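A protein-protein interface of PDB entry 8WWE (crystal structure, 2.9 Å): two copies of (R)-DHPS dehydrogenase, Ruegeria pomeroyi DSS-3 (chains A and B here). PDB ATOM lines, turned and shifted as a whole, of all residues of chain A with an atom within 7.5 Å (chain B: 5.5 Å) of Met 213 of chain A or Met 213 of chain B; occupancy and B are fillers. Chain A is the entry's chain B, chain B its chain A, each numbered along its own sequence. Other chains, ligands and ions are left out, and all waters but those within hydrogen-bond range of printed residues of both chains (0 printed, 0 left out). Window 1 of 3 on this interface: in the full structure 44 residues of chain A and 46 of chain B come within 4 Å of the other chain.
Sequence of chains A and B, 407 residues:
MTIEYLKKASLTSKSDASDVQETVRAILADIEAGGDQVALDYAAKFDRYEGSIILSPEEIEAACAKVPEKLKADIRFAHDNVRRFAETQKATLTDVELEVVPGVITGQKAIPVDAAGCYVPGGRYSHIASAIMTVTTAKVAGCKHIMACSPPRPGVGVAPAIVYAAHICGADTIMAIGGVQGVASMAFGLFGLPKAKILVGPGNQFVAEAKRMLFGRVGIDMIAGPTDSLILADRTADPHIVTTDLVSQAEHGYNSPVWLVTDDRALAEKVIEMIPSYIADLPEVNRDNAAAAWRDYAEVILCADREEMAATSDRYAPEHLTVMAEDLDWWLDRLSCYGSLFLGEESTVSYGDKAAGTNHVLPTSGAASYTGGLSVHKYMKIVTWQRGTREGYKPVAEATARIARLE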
ATOM      1  N   GLN A  21      18.891  19.041  17.554  1.00  0.00           N
ATOM      2  CA  GLN A  21      17.816  19.322  18.497  1.00  0.00           C
ATOM      3  C   GLN A  21      16.538  19.712  17.781  1.00  0.00           C
ATOM      4  O   GLN A  21      15.459  19.228  18.139  1.00  0.00           O
ATOM      5  CB  GLN A  21      18.228  20.427  19.464  1.00  0.00           C
ATOM      6  CG  GLN A  21      18.945  19.910  20.688  1.00  0.00           C
ATOM      7  CD  GLN A  21      20.464  19.802  20.487  1.00  0.00           C
ATOM      8  OE1 GLN A  21      21.042  20.476  19.621  1.00  0.00           O
ATOM      9  NE2 GLN A  21      21.119  18.979  21.324  1.00  0.00           N
ATOM     10  N   VAL A  24      14.847  16.677  16.152  1.00  0.00           N
ATOM     11  CA  VAL A  24      14.266  15.797  17.146  1.00  0.00           C
ATOM     12  C   VAL A  24      12.970  16.391  17.685  1.00  0.00           C
ATOM     13  O   VAL A  24      11.954  15.692  17.802  1.00  0.00           O
ATOM     14  CB  VAL A  24      15.284  15.530  18.261  1.00  0.00           C
ATOM     15  CG1 VAL A  24      14.660  14.653  19.287  1.00  0.00           C
ATOM     16  CG2 VAL A  24      16.488  14.859  17.687  1.00  0.00           C
ATOM     17  N   ARG A  25      12.992  17.685  18.044  1.00  0.00           N
ATOM     18  CA  ARG A  25      11.780  18.336  18.554  1.00  0.00           C
ATOM     19  C   ARG A  25      10.657  18.239  17.554  1.00  0.00           C
ATOM     20  O   ARG A  25       9.513  17.966  17.925  1.00  0.00           O
ATOM     21  CB  ARG A  25      12.037  19.794  18.882  1.00  0.00           C
ATOM     22  CG  ARG A  25      12.643  20.032  20.225  1.00  0.00           C
ATOM     23  CD  ARG A  25      12.427  21.459  20.543  1.00  0.00           C
ATOM     24  NE  ARG A  25      12.718  22.279  19.372  1.00  0.00           N
ATOM     25  CZ  ARG A  25      13.869  22.901  19.156  1.00  0.00           C
ATOM     26  NH1 ARG A  25      14.871  22.796  20.030  1.00  0.00           N
ATOM     27  NH2 ARG A  25      14.013  23.635  18.056  1.00  0.00           N
ATOM     28  N   LEU A  28       9.391  14.598  17.305  1.00  0.00           N
ATOM     29  CA  LEU A  28       8.672  14.274  18.531  1.00  0.00           C
ATOM     30  C   LEU A  28       7.302  14.952  18.575  1.00  0.00           C
ATOM     31  O   LEU A  28       6.299  14.315  18.898  1.00  0.00           O
ATOM     32  CB  LEU A  28       9.519  14.662  19.743  1.00  0.00           C
ATOM     33  CG  LEU A  28      10.622  13.666  20.146  1.00  0.00           C
ATOM     34  CD1 LEU A  28      11.596  14.266  21.192  1.00  0.00           C
ATOM     35  CD2 LEU A  28      10.070  12.276  20.594  1.00  0.00           C
ATOM     36  N   PHE A 206      20.684  11.363  17.074  1.00  0.00           N
ATOM     37  CA  PHE A 206      19.243  11.558  17.056  1.00  0.00           C
ATOM     38  C   PHE A 206      18.590  10.869  18.258  1.00  0.00           C
ATOM     39  O   PHE A 206      17.819  11.490  19.001  1.00  0.00           O
ATOM     40  CB  PHE A 206      18.657  11.013  15.747  1.00  0.00           C
ATOM     41  CG  PHE A 206      18.885  11.878  14.528  1.00  0.00           C
ATOM     42  CD1 PHE A 206      18.809  13.262  14.589  1.00  0.00           C
ATOM     43  CD2 PHE A 206      19.116  11.290  13.305  1.00  0.00           C
ATOM     44  CE1 PHE A 206      18.992  14.037  13.441  1.00  0.00           C
ATOM     45  CE2 PHE A 206      19.297  12.042  12.160  1.00  0.00           C
ATOM     46  CZ  PHE A 206      19.232  13.421  12.222  1.00  0.00           C
ATOM     47  N   VAL A 207      18.901   9.587  18.467  1.00  0.00           N
ATOM     48  CA  VAL A 207      18.332   8.829  19.577  1.00  0.00           C
ATOM     49  C   VAL A 207      18.743   9.434  20.917  1.00  0.00           C
ATOM     50  O   VAL A 207      17.931   9.566  21.843  1.00  0.00           O
ATOM     51  CB  VAL A 207      18.750   7.346  19.473  1.00  0.00           C
ATOM     52  CG1 VAL A 207      18.299   6.555  20.727  1.00  0.00           C
ATOM     53  CG2 VAL A 207      18.217   6.728  18.208  1.00  0.00           C
ATOM     54  N   ALA A 208      20.017   9.786  21.054  1.00  0.00           N
ATOM     55  CA  ALA A 208      20.462  10.318  22.334  1.00  0.00           C
ATOM     56  C   ALA A 208      19.744  11.632  22.667  1.00  0.00           C
ATOM     57  O   ALA A 208      19.406  11.881  23.827  1.00  0.00           O
ATOM     58  CB  ALA A 208      21.978  10.476  22.360  1.00  0.00           C
ATOM     59  N   GLU A 209      19.521  12.497  21.672  1.00  0.00           N
ATOM     60  CA  GLU A 209      18.788  13.735  21.934  1.00  0.00           C
ATOM     61  C   GLU A 209      17.328  13.458  22.222  1.00  0.00           C
ATOM     62  O   GLU A 209      16.734  14.140  23.053  1.00  0.00           O
ATOM     63  CB  GLU A 209      18.935  14.730  20.790  1.00  0.00           C
ATOM     64  CG  GLU A 209      18.092  15.984  20.941  1.00  0.00           C
ATOM     65  CD  GLU A 209      18.468  16.845  22.150  1.00  0.00           C
ATOM     66  OE1 GLU A 209      19.572  16.667  22.716  1.00  0.00           O
ATOM     67  OE2 GLU A 209      17.657  17.734  22.509  1.00  0.00           O
ATOM     68  N   ALA A 210      16.706  12.533  21.480  1.00  0.00           N
ATOM     69  CA  ALA A 210      15.314  12.200  21.762  1.00  0.00           C
ATOM     70  C   ALA A 210      15.160  11.707  23.180  1.00  0.00           C
ATOM     71  O   ALA A 210      14.206  12.086  23.878  1.00  0.00           O
ATOM     72  CB  ALA A 210      14.742  11.200  20.765  1.00  0.00           C
ATOM     73  N   LYS A 211      16.131  10.955  23.676  1.00  0.00           N
ATOM     74  CA  LYS A 211      15.921  10.443  25.022  1.00  0.00           C
ATOM     75  C   LYS A 211      16.316  11.484  26.058  1.00  0.00           C
ATOM     76  O   LYS A 211      15.738  11.509  27.145  1.00  0.00           O
ATOM     77  CB  LYS A 211      16.589   9.080  25.233  1.00  0.00           C
ATOM     78  CG  LYS A 211      18.062   8.887  25.007  1.00  0.00           C
ATOM     79  CD  LYS A 211      18.382   7.436  25.479  1.00  0.00           C
ATOM     80  CE  LYS A 211      19.878   7.146  25.681  1.00  0.00           C
ATOM     81  NZ  LYS A 211      20.125   5.776  26.255  1.00  0.00           N
ATOM     82  N   ARG A 212      17.282  12.356  25.746  1.00  0.00           N
ATOM     83  CA  ARG A 212      17.498  13.535  26.569  1.00  0.00           C
ATOM     84  C   ARG A 212      16.225  14.372  26.679  1.00  0.00           C
ATOM     85  O   ARG A 212      15.842  14.807  27.778  1.00  0.00           O
ATOM     86  CB  ARG A 212      18.636  14.355  25.988  1.00  0.00           C
ATOM     87  CG  ARG A 212      19.219  15.353  26.950  1.00  0.00           C
ATOM     88  CD  ARG A 212      20.040  16.371  26.190  1.00  0.00           C
ATOM     89  NE  ARG A 212      19.261  17.202  25.276  1.00  0.00           N
ATOM     90  CZ  ARG A 212      18.503  18.206  25.681  1.00  0.00           C
ATOM     91  NH1 ARG A 212      18.413  18.487  26.978  1.00  0.00           N
ATOM     92  NH2 ARG A 212      17.827  18.935  24.803  1.00  0.00           N
ATOM     93  N   MET A 213      15.535  14.576  25.562  1.00  0.00           N
ATOM     94  CA  MET A 213      14.346  15.415  25.581  1.00  0.00           C
ATOM     95  C   MET A 213      13.280  14.806  26.481  1.00  0.00           C
ATOM     96  O   MET A 213      12.748  15.468  27.387  1.00  0.00           O
ATOM     97  CB  MET A 213      13.793  15.574  24.166  1.00  0.00           C
ATOM     98  CG  MET A 213      14.529  16.581  23.287  1.00  0.00           C
ATOM     99  SD  MET A 213      14.250  18.287  23.780  1.00  0.00           S
ATOM    100  CE  MET A 213      12.466  18.258  23.829  1.00  0.00           C
ATOM    101  N   LEU A 214      13.012  13.512  26.297  1.00  0.00           N
ATOM    102  CA  LEU A 214      11.862  12.884  26.941  1.00  0.00           C
ATOM    103  C   LEU A 214      12.150  12.418  28.355  1.00  0.00           C
ATOM    104  O   LEU A 214      11.230  12.302  29.174  1.00  0.00           O
ATOM    105  CB  LEU A 214      11.360  11.736  26.066  1.00  0.00           C
ATOM    106  CG  LEU A 214      10.696  12.305  24.820  1.00  0.00           C
ATOM    107  CD1 LEU A 214      10.320  11.191  23.932  1.00  0.00           C
ATOM    108  CD2 LEU A 214       9.456  13.115  25.174  1.00  0.00           C
ATOM    109  N   PHE A 215      13.406  12.074  28.645  1.00  0.00           N
ATOM    110  CA  PHE A 215      13.776  11.450  29.906  1.00  0.00           C
ATOM    111  C   PHE A 215      14.729  12.277  30.735  1.00  0.00           C
ATOM    112  O   PHE A 215      14.935  11.953  31.910  1.00  0.00           O
ATOM    113  CB  PHE A 215      14.339  10.044  29.629  1.00  0.00           C
ATOM    114  CG  PHE A 215      13.294   9.108  29.057  1.00  0.00           C
ATOM    115  CD1 PHE A 215      12.267   8.591  29.872  1.00  0.00           C
ATOM    116  CD2 PHE A 215      13.249   8.837  27.710  1.00  0.00           C
ATOM    117  CE1 PHE A 215      11.273   7.774  29.353  1.00  0.00           C
ATOM    118  CE2 PHE A 215      12.251   8.021  27.200  1.00  0.00           C
ATOM    119  CZ  PHE A 215      11.268   7.491  28.032  1.00  0.00           C
ATOM    120  N   GLY A 216      15.258  13.371  30.176  1.00  0.00           N
ATOM    121  CA  GLY A 216      16.190  14.226  30.880  1.00  0.00           C
ATOM    122  C   GLY A 216      15.645  14.735  32.199  1.00  0.00           C
ATOM    123  O   GLY A 216      14.476  14.574  32.555  1.00  0.00           O
ATOM    124  N   ARG A 217      16.583  15.308  32.963  1.00  0.00           N
ATOM    125  CA  ARG A 217      16.353  15.948  34.254  1.00  0.00           C
ATOM    126  C   ARG A 217      16.204  14.828  35.266  1.00  0.00           C
ATOM    127  O   ARG A 217      17.082  13.959  35.335  1.00  0.00           O
ATOM    128  CB  ARG A 217      15.150  16.886  34.258  1.00  0.00           C
ATOM    129  CG  ARG A 217      15.116  17.808  35.470  1.00  0.00           C
ATOM    130  CD  ARG A 217      16.346  18.708  35.587  1.00  0.00           C
ATOM    131  NE  ARG A 217      16.069  19.889  36.406  1.00  0.00           N
ATOM    132  CZ  ARG A 217      15.354  20.941  35.997  1.00  0.00           C
ATOM    133  NH1 ARG A 217      14.824  20.966  34.773  1.00  0.00           N
ATOM    134  NH2 ARG A 217      15.155  21.969  36.817  1.00  0.00           N
ATOM    135  N   GLN B  21       6.524  18.787  31.658  1.00  0.00           N
ATOM    136  CA  GLN B  21       7.319  18.566  30.453  1.00  0.00           C
ATOM    137  C   GLN B  21       6.413  18.462  29.229  1.00  0.00           C
ATOM    138  O   GLN B  21       6.707  19.016  28.163  1.00  0.00           O
ATOM    139  CB  GLN B  21       8.138  17.286  30.600  1.00  0.00           C
ATOM    140  CG  GLN B  21       9.159  17.240  31.737  1.00  0.00           C
ATOM    141  CD  GLN B  21       9.982  15.938  31.720  1.00  0.00           C
ATOM    142  OE1 GLN B  21      11.230  15.961  31.734  1.00  0.00           O
ATOM    143  NE2 GLN B  21       9.278  14.792  31.705  1.00  0.00           N
ATOM    144  N   VAL B  24       5.127  21.948  28.362  1.00  0.00           N
ATOM    145  CA  VAL B  24       6.199  22.755  27.789  1.00  0.00           C
ATOM    146  C   VAL B  24       6.420  22.375  26.336  1.00  0.00           C
ATOM    147  O   VAL B  24       6.582  23.243  25.465  1.00  0.00           O
ATOM    148  CB  VAL B  24       7.480  22.592  28.608  1.00  0.00           C
ATOM    149  CG1 VAL B  24       8.432  23.674  28.231  1.00  0.00           C
ATOM    150  CG2 VAL B  24       7.141  22.639  30.062  1.00  0.00           C
ATOM    151  N   ARG B  25       6.466  21.065  26.060  1.00  0.00           N
ATOM    152  CA  ARG B  25       6.591  20.623  24.683  1.00  0.00           C
ATOM    153  C   ARG B  25       5.479  21.211  23.842  1.00  0.00           C
ATOM    154  O   ARG B  25       5.739  21.808  22.786  1.00  0.00           O
ATOM    155  CB  ARG B  25       6.565  19.101  24.596  1.00  0.00           C
ATOM    156  CG  ARG B  25       7.864  18.426  24.859  1.00  0.00           C
ATOM    157  CD  ARG B  25       7.913  17.074  24.212  1.00  0.00           C
ATOM    158  NE  ARG B  25       6.880  16.163  24.721  1.00  0.00           N
ATOM    159  CZ  ARG B  25       6.852  15.562  25.916  1.00  0.00           C
ATOM    160  NH1 ARG B  25       7.798  15.764  26.826  1.00  0.00           N
ATOM    161  NH2 ARG B  25       5.833  14.763  26.195  1.00  0.00           N
ATOM    162  N   LEU B  28       5.997  25.035  23.174  1.00  0.00           N
ATOM    163  CA  LEU B  28       7.140  25.289  22.313  1.00  0.00           C
ATOM    164  C   LEU B  28       6.795  24.908  20.894  1.00  0.00           C
ATOM    165  O   LEU B  28       7.088  25.655  19.964  1.00  0.00           O
ATOM    166  CB  LEU B  28       8.362  24.523  22.804  1.00  0.00           C
ATOM    167  CG  LEU B  28       9.127  25.061  24.005  1.00  0.00           C
ATOM    168  CD1 LEU B  28      10.131  24.029  24.471  1.00  0.00           C
ATOM    169  CD2 LEU B  28       9.814  26.364  23.677  1.00  0.00           C
ATOM    170  N   ALA B 208      12.420  26.646  33.585  1.00  0.00           N
ATOM    171  CA  ALA B 208      13.548  25.729  33.676  1.00  0.00           C
ATOM    172  C   ALA B 208      13.416  24.595  32.665  1.00  0.00           C
ATOM    173  O   ALA B 208      14.414  24.159  32.073  1.00  0.00           O
ATOM    174  CB  ALA B 208      13.668  25.187  35.093  1.00  0.00           C
ATOM    175  N   GLU B 209      12.200  24.083  32.474  1.00  0.00           N
ATOM    176  CA  GLU B 209      11.992  22.996  31.529  1.00  0.00           C
ATOM    177  C   GLU B 209      12.258  23.462  30.113  1.00  0.00           C
ATOM    178  O   GLU B 209      12.905  22.751  29.327  1.00  0.00           O
ATOM    179  CB  GLU B 209      10.583  22.434  31.675  1.00  0.00           C
ATOM    180  CG  GLU B 209      10.340  21.180  30.870  1.00  0.00           C
ATOM    181  CD  GLU B 209      11.346  20.095  31.180  1.00  0.00           C
ATOM    182  OE1 GLU B 209      11.702  19.357  30.228  1.00  0.00           O
ATOM    183  OE2 GLU B 209      11.745  19.980  32.375  1.00  0.00           O
ATOM    184  N   ALA B 210      11.707  24.625  29.751  1.00  0.00           N
ATOM    185  CA  ALA B 210      11.996  25.183  28.439  1.00  0.00           C
ATOM    186  C   ALA B 210      13.493  25.367  28.247  1.00  0.00           C
ATOM    187  O   ALA B 210      14.006  25.158  27.145  1.00  0.00           O
ATOM    188  CB  ALA B 210      11.248  26.494  28.217  1.00  0.00           C
ATOM    189  N   LYS B 211      14.229  25.702  29.308  1.00  0.00           N
ATOM    190  CA  LYS B 211      15.662  25.923  29.098  1.00  0.00           C
ATOM    191  C   LYS B 211      16.382  24.588  28.955  1.00  0.00           C
ATOM    192  O   LYS B 211      17.245  24.426  28.083  1.00  0.00           O
ATOM    193  CB  LYS B 211      16.311  26.703  30.241  1.00  0.00           C
ATOM    194  CG  LYS B 211      15.758  28.046  30.553  1.00  0.00           C
ATOM    195  CD  LYS B 211      16.333  28.557  31.868  1.00  0.00           C
ATOM    196  CE  LYS B 211      17.838  28.388  31.939  1.00  0.00           C
ATOM    197  NZ  LYS B 211      18.366  29.139  33.111  1.00  0.00           N
ATOM    198  N   ARG B 212      15.997  23.604  29.771  1.00  0.00           N
ATOM    199  CA  ARG B 212      16.544  22.267  29.643  1.00  0.00           C
ATOM    200  C   ARG B 212      16.384  21.737  28.221  1.00  0.00           C
ATOM    201  O   ARG B 212      17.337  21.211  27.628  1.00  0.00           O
ATOM    202  CB  ARG B 212      15.864  21.356  30.642  1.00  0.00           C
ATOM    203  CG  ARG B 212      16.653  20.104  30.915  1.00  0.00           C
ATOM    204  CD  ARG B 212      15.822  19.082  31.688  1.00  0.00           C
ATOM    205  NE  ARG B 212      14.611  18.693  30.977  1.00  0.00           N
ATOM    206  CZ  ARG B 212      14.620  18.051  29.815  1.00  0.00           C
ATOM    207  NH1 ARG B 212      15.773  17.732  29.235  1.00  0.00           N
ATOM    208  NH2 ARG B 212      13.481  17.715  29.223  1.00  0.00           N
ATOM    209  N   MET B 213      15.190  21.882  27.644  1.00  0.00           N
ATOM    210  CA  MET B 213      14.991  21.360  26.301  1.00  0.00           C
ATOM    211  C   MET B 213      15.762  22.154  25.274  1.00  0.00           C
ATOM    212  O   MET B 213      16.409  21.570  24.404  1.00  0.00           O
ATOM    213  CB  MET B 213      13.523  21.344  25.943  1.00  0.00           C
ATOM    214  CG  MET B 213      12.744  20.497  26.835  1.00  0.00           C
ATOM    215  SD  MET B 213      11.141  20.321  26.097  1.00  0.00           S
ATOM    216  CE  MET B 213      10.217  19.667  27.504  1.00  0.00           C
ATOM    217  N   LEU B 214      15.694  23.491  25.343  1.00  0.00           N
ATOM    218  CA  LEU B 214      16.226  24.323  24.263  1.00  0.00           C
ATOM    219  C   LEU B 214      17.733  24.575  24.392  1.00  0.00           C
ATOM    220  O   LEU B 214      18.442  24.645  23.388  1.00  0.00           O
ATOM    221  CB  LEU B 214      15.448  25.634  24.199  1.00  0.00           C
ATOM    222  CG  LEU B 214      14.003  25.564  23.668  1.00  0.00           C
ATOM    223  CD1 LEU B 214      13.421  26.916  23.626  1.00  0.00           C
ATOM    224  CD2 LEU B 214      13.915  24.989  22.297  1.00  0.00           C
ATOM    225  N   PHE B 215      18.255  24.739  25.608  1.00  0.00           N
ATOM    226  CA  PHE B 215      19.651  25.102  25.793  1.00  0.00           C
ATOM    227  C   PHE B 215      20.468  24.076  26.554  1.00  0.00           C
ATOM    228  O   PHE B 215      21.715  24.160  26.536  1.00  0.00           O
ATOM    229  CB  PHE B 215      19.739  26.463  26.497  1.00  0.00           C
ATOM    230  CG  PHE B 215      19.223  27.568  25.671  1.00  0.00           C
ATOM    231  CD1 PHE B 215      19.965  28.060  24.615  1.00  0.00           C
ATOM    232  CD2 PHE B 215      17.957  28.068  25.881  1.00  0.00           C
ATOM    233  CE1 PHE B 215      19.468  29.070  23.811  1.00  0.00           C
ATOM    234  CE2 PHE B 215      17.449  29.081  25.075  1.00  0.00           C
ATOM    235  CZ  PHE B 215      18.204  29.579  24.041  1.00  0.00           C
ATOM    236  N   GLY B 216      19.803  23.129  27.234  1.00  0.00           N
ATOM    237  CA  GLY B 216      20.511  22.060  27.890  1.00  0.00           C
ATOM    238  C   GLY B 216      21.249  21.167  26.910  1.00  0.00           C
ATOM    239  O   GLY B 216      21.013  21.179  25.689  1.00  0.00           O
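O of Met 213 of chain B lies within hydrogen-bond range of NH2 of Arg 212 of chain A.
O of Arg 212 of chain B lies within hydrogen-bond range of NH1 of Arg 212 of chain A (3.0 Å).
The guanidinium group (NH2) of Arg 212 of chain B sits at hydrogen-bond distance from the backbone carbonyl oxygen (O) of Met 213 of chain A (3.0 Å).
The side-chain carboxylate (OE2) of Glu 209 of chain A is in salt-bridge range of the guanidinium group (NH2) of Arg 212 of chain A, 2.6 Å away.
The guanidinium group (NH2) of Arg 212 of chain B lies within salt-bridge range of the side-chain carboxylate (OE1) of Glu 209 of chain B, 2.6 Å away.
The backbone carbonyl oxygen of Lys 211 of chain B sits at hydrogen-bond distance from the backbone NH of Gly 216 of chain B (3.0 Å).
The guanidinium group (NH2) of Arg 212 of chain A is in hydrogen-bond range of the side-chain sulfur (SD) of Met 213 of chain A, 3.8 Å away.
Among the printed residues, merely in contact across the chains: Arg 25 of chain A with Leu 214 of chain B, Arg 212 of chain A with Gly 216 of chain B, Met 213 of chain A with Met 213 of chain B, Leu 214 of chain A with Arg 25 of chain B, Gly 216 of chain A with Gln 21 of chain B, Gly 216 of chain A with Arg 212 of chain B, Arg 217 of chain A with Ala 208 of chain B and Arg 217 of chain A with Arg 212 of chain B.
Met 213 of chain A touches two residues of chain B.
Printed residues of chain A within 4 Å of Gly 216 of chain B: Arg 212 (3.9 Å).
Printed residues of chain B within 4 Å of Gly 216 of chain A: Gln 21 (3.6 Å) and Arg 212 (3.9 Å).
Printed residues of chain A within 4 Å of Arg 25 of chain B: Leu 214 (3.5 Å).
Of the printed residues of chain B, Arg 212 of chain A touches Arg 212 (3.0 Å), Met 213 (3.0 Å) and Gly 216 (3.9 Å).
The nearest residue of chain B that does not touch Met 213 of chain A is Gln 21 of chain B (4.6 Å).
Of the 13 printed residues of chain B, 7 touch a printed residue of chain A.
Of the 16 printed residues of chain A, 6 touch a printed residue of chain B.
Among the printed residues, 11 pairs touch across the chains.
Arg 25 of chain A touches Leu 214 of chain B, and with the chains exchanged Leu 214 of chain A touches Arg 25 of chain B.
Arg 212 of chain A touches its own counterpart, Arg 212 of chain B.
Arg 212 of chain A touches Met 213 of chain B, and with the chains exchanged Met 213 of chain A touches Arg 212 of chain B.
Met 213 of chain A touches its own counterpart, Met 213 of chain B.
Positions printed for both chains: 21, 24, 25, 28, 208, 209, 210, 211, 212, 213, 214, 215 and 216.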
